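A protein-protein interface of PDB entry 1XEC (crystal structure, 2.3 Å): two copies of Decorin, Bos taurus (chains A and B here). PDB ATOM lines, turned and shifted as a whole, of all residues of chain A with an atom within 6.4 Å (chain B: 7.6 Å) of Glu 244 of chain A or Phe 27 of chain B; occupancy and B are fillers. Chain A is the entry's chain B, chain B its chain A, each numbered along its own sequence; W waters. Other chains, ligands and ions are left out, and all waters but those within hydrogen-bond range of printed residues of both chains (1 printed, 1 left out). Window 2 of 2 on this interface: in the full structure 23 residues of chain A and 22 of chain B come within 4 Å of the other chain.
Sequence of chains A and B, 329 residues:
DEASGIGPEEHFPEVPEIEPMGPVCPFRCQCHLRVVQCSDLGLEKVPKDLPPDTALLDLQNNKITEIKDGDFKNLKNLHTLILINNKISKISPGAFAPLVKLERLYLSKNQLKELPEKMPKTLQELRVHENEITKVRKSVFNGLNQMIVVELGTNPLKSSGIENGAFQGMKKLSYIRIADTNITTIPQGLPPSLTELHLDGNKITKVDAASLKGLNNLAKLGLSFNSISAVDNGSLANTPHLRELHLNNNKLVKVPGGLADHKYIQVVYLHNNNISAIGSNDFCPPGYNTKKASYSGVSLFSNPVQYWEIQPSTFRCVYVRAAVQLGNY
Of the 20 printed residues of chain A, 4 touch a printed residue of chain B. Hydrophobic or aromatic side chains of chain A within 4 Å of the printed part of chain B: His 198 and His 246. Among the printed residues, no Asp or Glu carboxylate lies within 4 Å of a Lys or Arg side-chain nitrogen of the other chain.
No position is printed for both chains. Of the 5 pairs that touch across the chains among the printed residues, none has its exchanged pair printed and touching as well.
O of Arg 28 of chain B is in hydrogen-bond range of NE2 of Gln 30 of chain B, at 2.7 Å. NE2 of His 198 of chain A is in hydrogen-bond range of OE2 of Glu 196 of chain A (2.9 Å). The side-chain carboxylate (OE1) of Glu 196 of chain A is in salt-bridge range of the side-chain amino group (NZ) of Lys 220 of chain A (3.9 Å). O of Leu 221 of chain A lies within hydrogen-bond range of N of His 246 of chain A (3.1 Å). O of His 246 of chain A sits at hydrogen-bond distance from N of Leu 223 of chain A, 3.0 Å away. The side-chain sulfur (SG) of Cys 31 of chain B is disulfide-bonded to the side-chain sulfur (SG) of Cys 25 of chain B, at 2.0 Å.
CZ of Phe 27 of chain B touches CE1 of His 198 of chain A, at 3.7 Å. His 198 of chain A touches Arg 28 of chain B (ND1 to CG, 3.6 Å). Lys 220 of chain A touches Phe 27 of chain B (CD to CE2, 3.9 Å). Glu 244 of chain A touches Phe 27 of chain B (OE2 to CD2, 3.2 Å). Phe 27 of chain B touches His 246 of chain A.
Water W1 lies within hydrogen-bond range of the backbone carbonyl oxygen of Cys 29 of chain B and the side-chain carboxylate of Glu 196 of chain A.
Of the printed residues of chain A, Phe 27 of chain B touches His 198 (3.7 Å), Lys 220 (3.9 Å), Glu 244 (3.2 Å) and His 246 (3.2 Å). Of the printed residues of chain B, Lys 220 of chain A touches Phe 27. Printed residues of chain B within 4 Å of His 198 of chain A: Phe 27 (3.7 Å) and Arg 28 (3.6 Å). Of the printed residues of chain B, His 246 of chain A touches Phe 27 (3.2 Å). Printed residues of chain A within 4 Å of Arg 28 of chain B: His 198. The nearest residue of chain B that does not touch Glu 244 of chain A is Cys 25 of chain B (6.4 Å). The nearest printed residue of chain A that does not touch Phe 27 of chain B is Gly 222 of chain A (4.02 Å).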
ATOM      1  N   GLU A 196      20.228   2.781   5.196  1.00  0.00           N
ATOM      2  CA  GLU A 196      20.349   3.191   6.594  1.00  0.00           C
ATOM      3  C   GLU A 196      21.623   2.689   7.261  1.00  0.00           C
ATOM      4  O   GLU A 196      21.939   1.498   7.215  1.00  0.00           O
ATOM      5  CB  GLU A 196      19.145   2.710   7.404  1.00  0.00           C
ATOM      6  CG  GLU A 196      17.821   3.040   6.776  1.00  0.00           C
ATOM      7  CD  GLU A 196      16.681   2.990   7.770  1.00  0.00           C
ATOM      8  OE1 GLU A 196      15.516   2.876   7.327  1.00  0.00           O
ATOM      9  OE2 GLU A 196      16.944   3.077   8.992  1.00  0.00           O
ATOM     10  N   LEU A 197      22.350   3.616   7.875  1.00  0.00           N
ATOM     11  CA  LEU A 197      23.585   3.304   8.581  1.00  0.00           C
ATOM     12  C   LEU A 197      23.456   3.819  10.015  1.00  0.00           C
ATOM     13  O   LEU A 197      23.398   5.025  10.254  1.00  0.00           O
ATOM     14  CB  LEU A 197      24.770   3.974   7.884  1.00  0.00           C
ATOM     15  CG  LEU A 197      26.146   3.783   8.536  1.00  0.00           C
ATOM     16  CD1 LEU A 197      26.418   2.309   8.775  1.00  0.00           C
ATOM     17  CD2 LEU A 197      27.214   4.377   7.623  1.00  0.00           C
ATOM     18  N   HIS A 198      23.399   2.908  10.972  1.00  0.00           N
ATOM     19  CA  HIS A 198      23.249   3.313  12.363  1.00  0.00           C
ATOM     20  C   HIS A 198      24.467   2.954  13.185  1.00  0.00           C
ATOM     21  O   HIS A 198      24.763   1.782  13.381  1.00  0.00           O
ATOM     22  CB  HIS A 198      22.005   2.658  12.969  1.00  0.00           C
ATOM     23  CG  HIS A 198      20.726   3.112  12.343  1.00  0.00           C
ATOM     24  ND1 HIS A 198      20.256   4.401  12.466  1.00  0.00           N
ATOM     25  CD2 HIS A 198      19.853   2.469  11.532  1.00  0.00           C
ATOM     26  CE1 HIS A 198      19.152   4.536  11.753  1.00  0.00           C
ATOM     27  NE2 HIS A 198      18.886   3.377  11.175  1.00  0.00           N
ATOM     28  N   ALA A 219      19.862   7.236   3.099  1.00  0.00           N
ATOM     29  CA  ALA A 219      18.838   8.211   3.436  1.00  0.00           C
ATOM     30  C   ALA A 219      18.894   8.559   4.922  1.00  0.00           C
ATOM     31  O   ALA A 219      18.452   9.630   5.325  1.00  0.00           O
ATOM     32  CB  ALA A 219      17.452   7.661   3.068  1.00  0.00           C
ATOM     33  N   LYS A 220      19.432   7.656   5.734  1.00  0.00           N
ATOM     34  CA  LYS A 220      19.532   7.898   7.172  1.00  0.00           C
ATOM     35  C   LYS A 220      20.903   7.534   7.728  1.00  0.00           C
ATOM     36  O   LYS A 220      21.402   6.431   7.505  1.00  0.00           O
ATOM     37  CB  LYS A 220      18.465   7.102   7.932  1.00  0.00           C
ATOM     38  CG  LYS A 220      17.028   7.443   7.559  1.00  0.00           C
ATOM     39  CD  LYS A 220      16.061   6.579   8.343  1.00  0.00           C
ATOM     40  CE  LYS A 220      14.611   6.863   7.973  1.00  0.00           C
ATOM     41  NZ  LYS A 220      13.703   6.036   8.818  1.00  0.00           N
ATOM     42  N   LEU A 221      21.498   8.473   8.460  1.00  0.00           N
ATOM     43  CA  LEU A 221      22.804   8.273   9.074  1.00  0.00           C
ATOM     44  C   LEU A 221      22.687   8.547  10.581  1.00  0.00           C
ATOM     45  O   LEU A 221      22.450   9.676  11.003  1.00  0.00           O
ATOM     46  CB  LEU A 221      23.831   9.218   8.435  1.00  0.00           C
ATOM     47  CG  LEU A 221      25.262   9.179   8.992  1.00  0.00           C
ATOM     48  CD1 LEU A 221      25.850   7.789   8.835  1.00  0.00           C
ATOM     49  CD2 LEU A 221      26.114  10.199   8.263  1.00  0.00           C
ATOM     50  N   GLY A 222      22.839   7.499  11.384  1.00  0.00           N
ATOM     51  CA  GLY A 222      22.736   7.649  12.824  1.00  0.00           C
ATOM     52  C   GLY A 222      24.093   7.589  13.493  1.00  0.00           C
ATOM     53  O   GLY A 222      24.734   6.532  13.517  1.00  0.00           O
ATOM     54  N   LEU A 223      24.522   8.721  14.048  1.00  0.00           N
ATOM     55  CA  LEU A 223      25.822   8.823  14.715  1.00  0.00           C
ATOM     56  C   LEU A 223      25.711   9.374  16.135  1.00  0.00           C
ATOM     57  O   LEU A 223      26.725   9.677  16.766  1.00  0.00           O
ATOM     58  CB  LEU A 223      26.747   9.731  13.901  1.00  0.00           C
ATOM     59  CG  LEU A 223      27.169   9.249  12.510  1.00  0.00           C
ATOM     60  CD1 LEU A 223      27.642  10.418  11.686  1.00  0.00           C
ATOM     61  CD2 LEU A 223      28.251   8.198  12.632  1.00  0.00           C
ATOM     62  N   SER A 224      24.496   9.492  16.649  1.00  0.00           N
ATOM     63  CA  SER A 224      24.322  10.045  17.984  1.00  0.00           C
ATOM     64  C   SER A 224      25.031   9.256  19.103  1.00  0.00           C
ATOM     65  O   SER A 224      25.332   8.067  18.960  1.00  0.00           O
ATOM     66  CB  SER A 224      22.830  10.181  18.293  1.00  0.00           C
ATOM     67  OG  SER A 224      22.269   8.933  18.624  1.00  0.00           O
ATOM     68  N   HIS A 241      21.912  12.025  -1.142  1.00  0.00           N
ATOM     69  CA  HIS A 241      20.481  11.883  -0.887  1.00  0.00           C
ATOM     70  C   HIS A 241      20.093  11.690   0.578  1.00  0.00           C
ATOM     71  O   HIS A 241      18.958  11.323   0.883  1.00  0.00           O
ATOM     72  CB  HIS A 241      19.919  10.747  -1.743  1.00  0.00           C
ATOM     73  CG  HIS A 241      20.191  10.924  -3.203  1.00  0.00           C
ATOM     74  ND1 HIS A 241      21.121  10.169  -3.884  1.00  0.00           N
ATOM     75  CD2 HIS A 241      19.736  11.846  -4.085  1.00  0.00           C
ATOM     76  CE1 HIS A 241      21.232  10.621  -5.121  1.00  0.00           C
ATOM     77  NE2 HIS A 241      20.402  11.639  -5.267  1.00  0.00           N
ATOM     78  N   LEU A 242      21.026  11.963   1.485  1.00  0.00           N
ATOM     79  CA  LEU A 242      20.755  11.819   2.909  1.00  0.00           C
ATOM     80  C   LEU A 242      19.557  12.679   3.305  1.00  0.00           C
ATOM     81  O   LEU A 242      19.470  13.850   2.933  1.00  0.00           O
ATOM     82  CB  LEU A 242      21.985  12.235   3.723  1.00  0.00           C
ATOM     83  CG  LEU A 242      21.915  11.944   5.224  1.00  0.00           C
ATOM     84  CD1 LEU A 242      21.858  10.437   5.430  1.00  0.00           C
ATOM     85  CD2 LEU A 242      23.127  12.541   5.943  1.00  0.00           C
ATOM     86  N   ARG A 243      18.628  12.104   4.057  1.00  0.00           N
ATOM     87  CA  ARG A 243      17.463  12.865   4.483  1.00  0.00           C
ATOM     88  C   ARG A 243      17.482  13.133   5.990  1.00  0.00           C
ATOM     89  O   ARG A 243      17.103  14.210   6.440  1.00  0.00           O
ATOM     90  CB  ARG A 243      16.165  12.140   4.090  1.00  0.00           C
ATOM     91  CG  ARG A 243      14.911  12.933   4.465  1.00  0.00           C
ATOM     92  CD  ARG A 243      13.601  12.305   3.968  1.00  0.00           C
ATOM     93  NE  ARG A 243      13.420  10.936   4.447  1.00  0.00           N
ATOM     94  CZ  ARG A 243      13.849   9.852   3.805  1.00  0.00           C
ATOM     95  NH1 ARG A 243      14.484   9.957   2.640  1.00  0.00           N
ATOM     96  NH2 ARG A 243      13.652   8.652   4.336  1.00  0.00           N
ATOM     97  N   GLU A 244      17.940  12.156   6.761  1.00  0.00           N
ATOM     98  CA  GLU A 244      17.990  12.292   8.210  1.00  0.00           C
ATOM     99  C   GLU A 244      19.390  12.080   8.766  1.00  0.00           C
ATOM    100  O   GLU A 244      20.007  11.039   8.545  1.00  0.00           O
ATOM    101  CB  GLU A 244      17.029  11.306   8.861  1.00  0.00           C
ATOM    102  CG  GLU A 244      15.583  11.517   8.452  1.00  0.00           C
ATOM    103  CD  GLU A 244      14.622  10.609   9.191  1.00  0.00           C
ATOM    104  OE1 GLU A 244      13.437  10.556   8.805  1.00  0.00           O
ATOM    105  OE2 GLU A 244      15.051   9.951  10.160  1.00  0.00           O
ATOM    106  N   LEU A 245      19.878  13.078   9.491  1.00  0.00           N
ATOM    107  CA  LEU A 245      21.204  13.022  10.096  1.00  0.00           C
ATOM    108  C   LEU A 245      21.104  13.291  11.608  1.00  0.00           C
ATOM    109  O   LEU A 245      20.789  14.409  12.035  1.00  0.00           O
ATOM    110  CB  LEU A 245      22.115  14.061   9.435  1.00  0.00           C
ATOM    111  CG  LEU A 245      23.548  14.218   9.951  1.00  0.00           C
ATOM    112  CD1 LEU A 245      24.321  12.915   9.803  1.00  0.00           C
ATOM    113  CD2 LEU A 245      24.234  15.323   9.164  1.00  0.00           C
ATOM    114  N   HIS A 246      21.348  12.257  12.406  1.00  0.00           N
ATOM    115  CA  HIS A 246      21.301  12.400  13.858  1.00  0.00           C
ATOM    116  C   HIS A 246      22.727  12.471  14.379  1.00  0.00           C
ATOM    117  O   HIS A 246      23.474  11.486  14.319  1.00  0.00           O
ATOM    118  CB  HIS A 246      20.562  11.222  14.512  1.00  0.00           C
ATOM    119  CG  HIS A 246      19.100  11.164  14.183  1.00  0.00           C
ATOM    120  ND1 HIS A 246      18.185  10.511  14.976  1.00  0.00           N
ATOM    121  CD2 HIS A 246      18.394  11.697  13.158  1.00  0.00           C
ATOM    122  CE1 HIS A 246      16.977  10.652  14.461  1.00  0.00           C
ATOM    123  NE2 HIS A 246      17.076  11.368  13.359  1.00  0.00           N
ATOM    124  N   TYR A 264      18.998  17.235  -0.291  1.00  0.00           N
ATOM    125  CA  TYR A 264      18.038  16.308   0.287  1.00  0.00           C
ATOM    126  C   TYR A 264      17.912  16.302   1.802  1.00  0.00           C
ATOM    127  O   TYR A 264      16.878  15.893   2.328  1.00  0.00           O
ATOM    128  CB  TYR A 264      18.335  14.886  -0.202  1.00  0.00           C
ATOM    129  CG  TYR A 264      18.039  14.679  -1.673  1.00  0.00           C
ATOM    130  CD1 TYR A 264      18.844  15.259  -2.657  1.00  0.00           C
ATOM    131  CD2 TYR A 264      16.944  13.917  -2.082  1.00  0.00           C
ATOM    132  CE1 TYR A 264      18.564  15.085  -4.014  1.00  0.00           C
ATOM    133  CE2 TYR A 264      16.653  13.736  -3.435  1.00  0.00           C
ATOM    134  CZ  TYR A 264      17.468  14.320  -4.393  1.00  0.00           C
ATOM    135  OH  TYR A 264      17.198  14.129  -5.725  1.00  0.00           O
ATOM    136  N   ILE A 265      18.943  16.757   2.507  1.00  0.00           N
ATOM    137  CA  ILE A 265      18.897  16.760   3.967  1.00  0.00           C
ATOM    138  C   ILE A 265      17.653  17.465   4.496  1.00  0.00           C
ATOM    139  O   ILE A 265      17.358  18.586   4.105  1.00  0.00           O
ATOM    140  CB  ILE A 265      20.150  17.432   4.571  1.00  0.00           C
ATOM    141  CG1 ILE A 265      20.147  17.240   6.087  1.00  0.00           C
ATOM    142  CG2 ILE A 265      20.192  18.899   4.213  1.00  0.00           C
ATOM    143  CD1 ILE A 265      20.166  15.796   6.495  1.00  0.00           C
ATOM    144  N   GLN A 266      16.927  16.807   5.393  1.00  0.00           N
ATOM    145  CA  GLN A 266      15.715  17.390   5.952  1.00  0.00           C
ATOM    146  C   GLN A 266      15.652  17.382   7.480  1.00  0.00           C
ATOM    147  O   GLN A 266      14.991  18.225   8.091  1.00  0.00           O
ATOM    148  CB  GLN A 266      14.493  16.665   5.390  1.00  0.00           C
ATOM    149  CG  GLN A 266      14.215  16.968   3.927  1.00  0.00           C
ATOM    150  CD  GLN A 266      12.855  16.459   3.481  1.00  0.00           C
ATOM    151  OE1 GLN A 266      12.677  15.266   3.219  1.00  0.00           O
ATOM    152  NE2 GLN A 266      11.880  17.364   3.406  1.00  0.00           N
ATOM    153  N   VAL A 267      16.323  16.416   8.094  1.00  0.00           N
ATOM    154  CA  VAL A 267      16.335  16.308   9.541  1.00  0.00           C
ATOM    155  C   VAL A 267      17.762  16.353  10.063  1.00  0.00           C
ATOM    156  O   VAL A 267      18.596  15.525   9.689  1.00  0.00           O
ATOM    157  CB  VAL A 267      15.682  14.996  10.003  1.00  0.00           C
ATOM    158  CG1 VAL A 267      15.696  14.912  11.522  1.00  0.00           C
ATOM    159  CG2 VAL A 267      14.261  14.924   9.489  1.00  0.00           C
ATOM    160  N   VAL A 268      18.039  17.322  10.927  1.00  0.00           N
ATOM    161  CA  VAL A 268      19.373  17.458  11.494  1.00  0.00           C
ATOM    162  C   VAL A 268      19.321  17.659  13.003  1.00  0.00           C
ATOM    163  O   VAL A 268      18.979  18.738  13.481  1.00  0.00           O
ATOM    164  CB  VAL A 268      20.137  18.645  10.857  1.00  0.00           C
ATOM    165  CG1 VAL A 268      21.585  18.652  11.337  1.00  0.00           C
ATOM    166  CG2 VAL A 268      20.093  18.542   9.344  1.00  0.00           C
ATOM    167  N   VAL B  24       4.653   6.495  10.475  1.00  0.00           N
ATOM    168  CA  VAL B  24       6.071   6.776  10.660  1.00  0.00           C
ATOM    169  C   VAL B  24       6.803   5.550  11.208  1.00  0.00           C
ATOM    170  O   VAL B  24       6.237   4.770  11.967  1.00  0.00           O
ATOM    171  CB  VAL B  24       6.262   7.942  11.659  1.00  0.00           C
ATOM    172  CG1 VAL B  24       7.752   8.258  11.828  1.00  0.00           C
ATOM    173  CG2 VAL B  24       5.495   9.165  11.181  1.00  0.00           C
ATOM    174  N   CYS B  25       8.055   5.369  10.814  1.00  0.00           N
ATOM    175  CA  CYS B  25       8.834   4.250  11.327  1.00  0.00           C
ATOM    176  C   CYS B  25       9.842   4.864  12.299  1.00  0.00           C
ATOM    177  O   CYS B  25      10.637   5.718  11.920  1.00  0.00           O
ATOM    178  CB  CYS B  25       9.561   3.517  10.187  1.00  0.00           C
ATOM    179  SG  CYS B  25      10.334   1.921  10.654  1.00  0.00           S
ATOM    180  N   PRO B  26       9.806   4.451  13.573  1.00  0.00           N
ATOM    181  CA  PRO B  26      10.763   5.029  14.524  1.00  0.00           C
ATOM    182  C   PRO B  26      12.203   4.883  14.013  1.00  0.00           C
ATOM    183  O   PRO B  26      12.560   3.870  13.411  1.00  0.00           O
ATOM    184  CB  PRO B  26      10.511   4.226  15.806  1.00  0.00           C
ATOM    185  CG  PRO B  26       9.068   3.790  15.663  1.00  0.00           C
ATOM    186  CD  PRO B  26       8.979   3.414  14.210  1.00  0.00           C
ATOM    187  N   PHE B  27      13.018   5.905  14.251  1.00  0.00           N
ATOM    188  CA  PHE B  27      14.408   5.906  13.823  1.00  0.00           C
ATOM    189  C   PHE B  27      15.108   4.681  14.400  1.00  0.00           C
ATOM    190  O   PHE B  27      15.028   4.420  15.605  1.00  0.00           O
ATOM    191  CB  PHE B  27      15.093   7.194  14.301  1.00  0.00           C
ATOM    192  CG  PHE B  27      16.375   7.510  13.585  1.00  0.00           C
ATOM    193  CD1 PHE B  27      17.602   7.394  14.236  1.00  0.00           C
ATOM    194  CD2 PHE B  27      16.355   7.941  12.258  1.00  0.00           C
ATOM    195  CE1 PHE B  27      18.793   7.706  13.580  1.00  0.00           C
ATOM    196  CE2 PHE B  27      17.544   8.256  11.590  1.00  0.00           C
ATOM    197  CZ  PHE B  27      18.767   8.138  12.259  1.00  0.00           C
ATOM    198  N   ARG B  28      15.776   3.933  13.524  1.00  0.00           N
ATOM    199  CA  ARG B  28      16.501   2.714  13.871  1.00  0.00           C
ATOM    200  C   ARG B  28      15.644   1.454  13.796  1.00  0.00           C
ATOM    201  O   ARG B  28      16.183   0.348  13.752  1.00  0.00           O
ATOM    202  CB  ARG B  28      17.127   2.820  15.261  1.00  0.00           C
ATOM    203  CG  ARG B  28      18.236   3.850  15.370  1.00  0.00           C
ATOM    204  CD  ARG B  28      18.717   3.954  16.800  1.00  0.00           C
ATOM    205  NE  ARG B  28      17.607   4.257  17.694  1.00  0.00           N
ATOM    206  CZ  ARG B  28      17.676   4.176  19.019  1.00  0.00           C
ATOM    207  NH1 ARG B  28      18.807   3.803  19.607  1.00  0.00           N
ATOM    208  NH2 ARG B  28      16.608   4.454  19.753  1.00  0.00           N
ATOM    209  N   CYS B  29      14.321   1.601  13.790  1.00  0.00           N
ATOM    210  CA  CYS B  29      13.459   0.424  13.693  1.00  0.00           C
ATOM    211  C   CYS B  29      13.377   0.009  12.227  1.00  0.00           C
ATOM    212  O   CYS B  29      13.771   0.754  11.331  1.00  0.00           O
ATOM    213  CB  CYS B  29      12.027   0.699  14.187  1.00  0.00           C
ATOM    214  SG  CYS B  29      11.742   1.152  15.942  1.00  0.00           S
ATOM    215  N   GLN B  30      12.870  -1.192  11.990  1.00  0.00           N
ATOM    216  CA  GLN B  30      12.711  -1.681  10.637  1.00  0.00           C
ATOM    217  C   GLN B  30      11.236  -1.991  10.455  1.00  0.00           C
ATOM    218  O   GLN B  30      10.668  -2.802  11.178  1.00  0.00           O
ATOM    219  CB  GLN B  30      13.571  -2.933  10.404  1.00  0.00           C
ATOM    220  CG  GLN B  30      15.058  -2.728  10.710  1.00  0.00           C
ATOM    221  CD  GLN B  30      15.446  -3.181  12.121  1.00  0.00           C
ATOM    222  OE1 GLN B  30      15.629  -4.370  12.369  1.00  0.00           O
ATOM    223  NE2 GLN B  30      15.564  -2.232  13.046  1.00  0.00           N
ATOM    224  N   CYS B  31      10.611  -1.314   9.503  1.00  0.00           N
ATOM    225  CA  CYS B  31       9.193  -1.508   9.222  1.00  0.00           C
ATOM    226  C   CYS B  31       9.083  -2.116   7.828  1.00  0.00           C
ATOM    227  O   CYS B  31       9.173  -1.420   6.825  1.00  0.00           O
ATOM    228  CB  CYS B  31       8.475  -0.160   9.307  1.00  0.00           C
ATOM    229  SG  CYS B  31       8.747   0.652  10.923  1.00  0.00           S
ATOM    230  N   CYS B  38      11.521  -3.325  16.246  1.00  0.00           N
ATOM    231  CA  CYS B  38      12.130  -2.268  17.045  1.00  0.00           C
ATOM    232  C   CYS B  38      12.970  -2.791  18.207  1.00  0.00           C
ATOM    233  O   CYS B  38      13.169  -2.091  19.196  1.00  0.00           O
ATOM    234  CB  CYS B  38      11.051  -1.375  17.627  1.00  0.00           C
ATOM    235  SG  CYS B  38      10.263  -0.120  16.568  1.00  0.00           S
ATOM    236  N   LEU B  41      16.897  -1.440  20.938  1.00  0.00           N
ATOM    237  CA  LEU B  41      17.145  -0.016  20.731  1.00  0.00           C
ATOM    238  C   LEU B  41      17.126   0.866  21.972  1.00  0.00           C
ATOM    239  O   LEU B  41      17.261   2.083  21.868  1.00  0.00           O
ATOM    240  CB  LEU B  41      16.142   0.549  19.718  1.00  0.00           C
ATOM    241  CG  LEU B  41      16.135  -0.113  18.343  1.00  0.00           C
ATOM    242  CD1 LEU B  41      15.070   0.549  17.482  1.00  0.00           C
ATOM    243  CD2 LEU B  41      17.511   0.007  17.691  1.00  0.00           C
ATOM    244  N   LEU B  43      14.644   1.720  23.717  1.00  0.00           N
ATOM    245  CA  LEU B  43      13.468   2.597  23.742  1.00  0.00           C
ATOM    246  C   LEU B  43      12.896   2.721  25.146  1.00  0.00           C
ATOM    247  O   LEU B  43      12.816   1.736  25.868  1.00  0.00           O
ATOM    248  CB  LEU B  43      12.386   2.076  22.794  1.00  0.00           C
ATOM    249  CG  LEU B  43      12.765   2.098  21.312  1.00  0.00           C
ATOM    250  CD1 LEU B  43      11.653   1.484  20.492  1.00  0.00           C
ATOM    251  CD2 LEU B  43      13.032   3.526  20.871  1.00  0.00           C
ATOM    252  N   PRO B  47       6.504   3.277  20.915  1.00  0.00           N
ATOM    253  CA  PRO B  47       6.435   4.286  19.856  1.00  0.00           C
ATOM    254  C   PRO B  47       5.022   4.362  19.292  1.00  0.00           C
ATOM    255  O   PRO B  47       4.297   3.371  19.287  1.00  0.00           O
ATOM    256  CB  PRO B  47       7.446   3.777  18.837  1.00  0.00           C
ATOM    257  CG  PRO B  47       7.319   2.301  18.969  1.00  0.00           C
ATOM    258  CD  PRO B  47       7.278   2.105  20.468  1.00  0.00           C
HETATM  259  O   HOH W   1      14.361   0.125   8.343  1.00  0.00           O
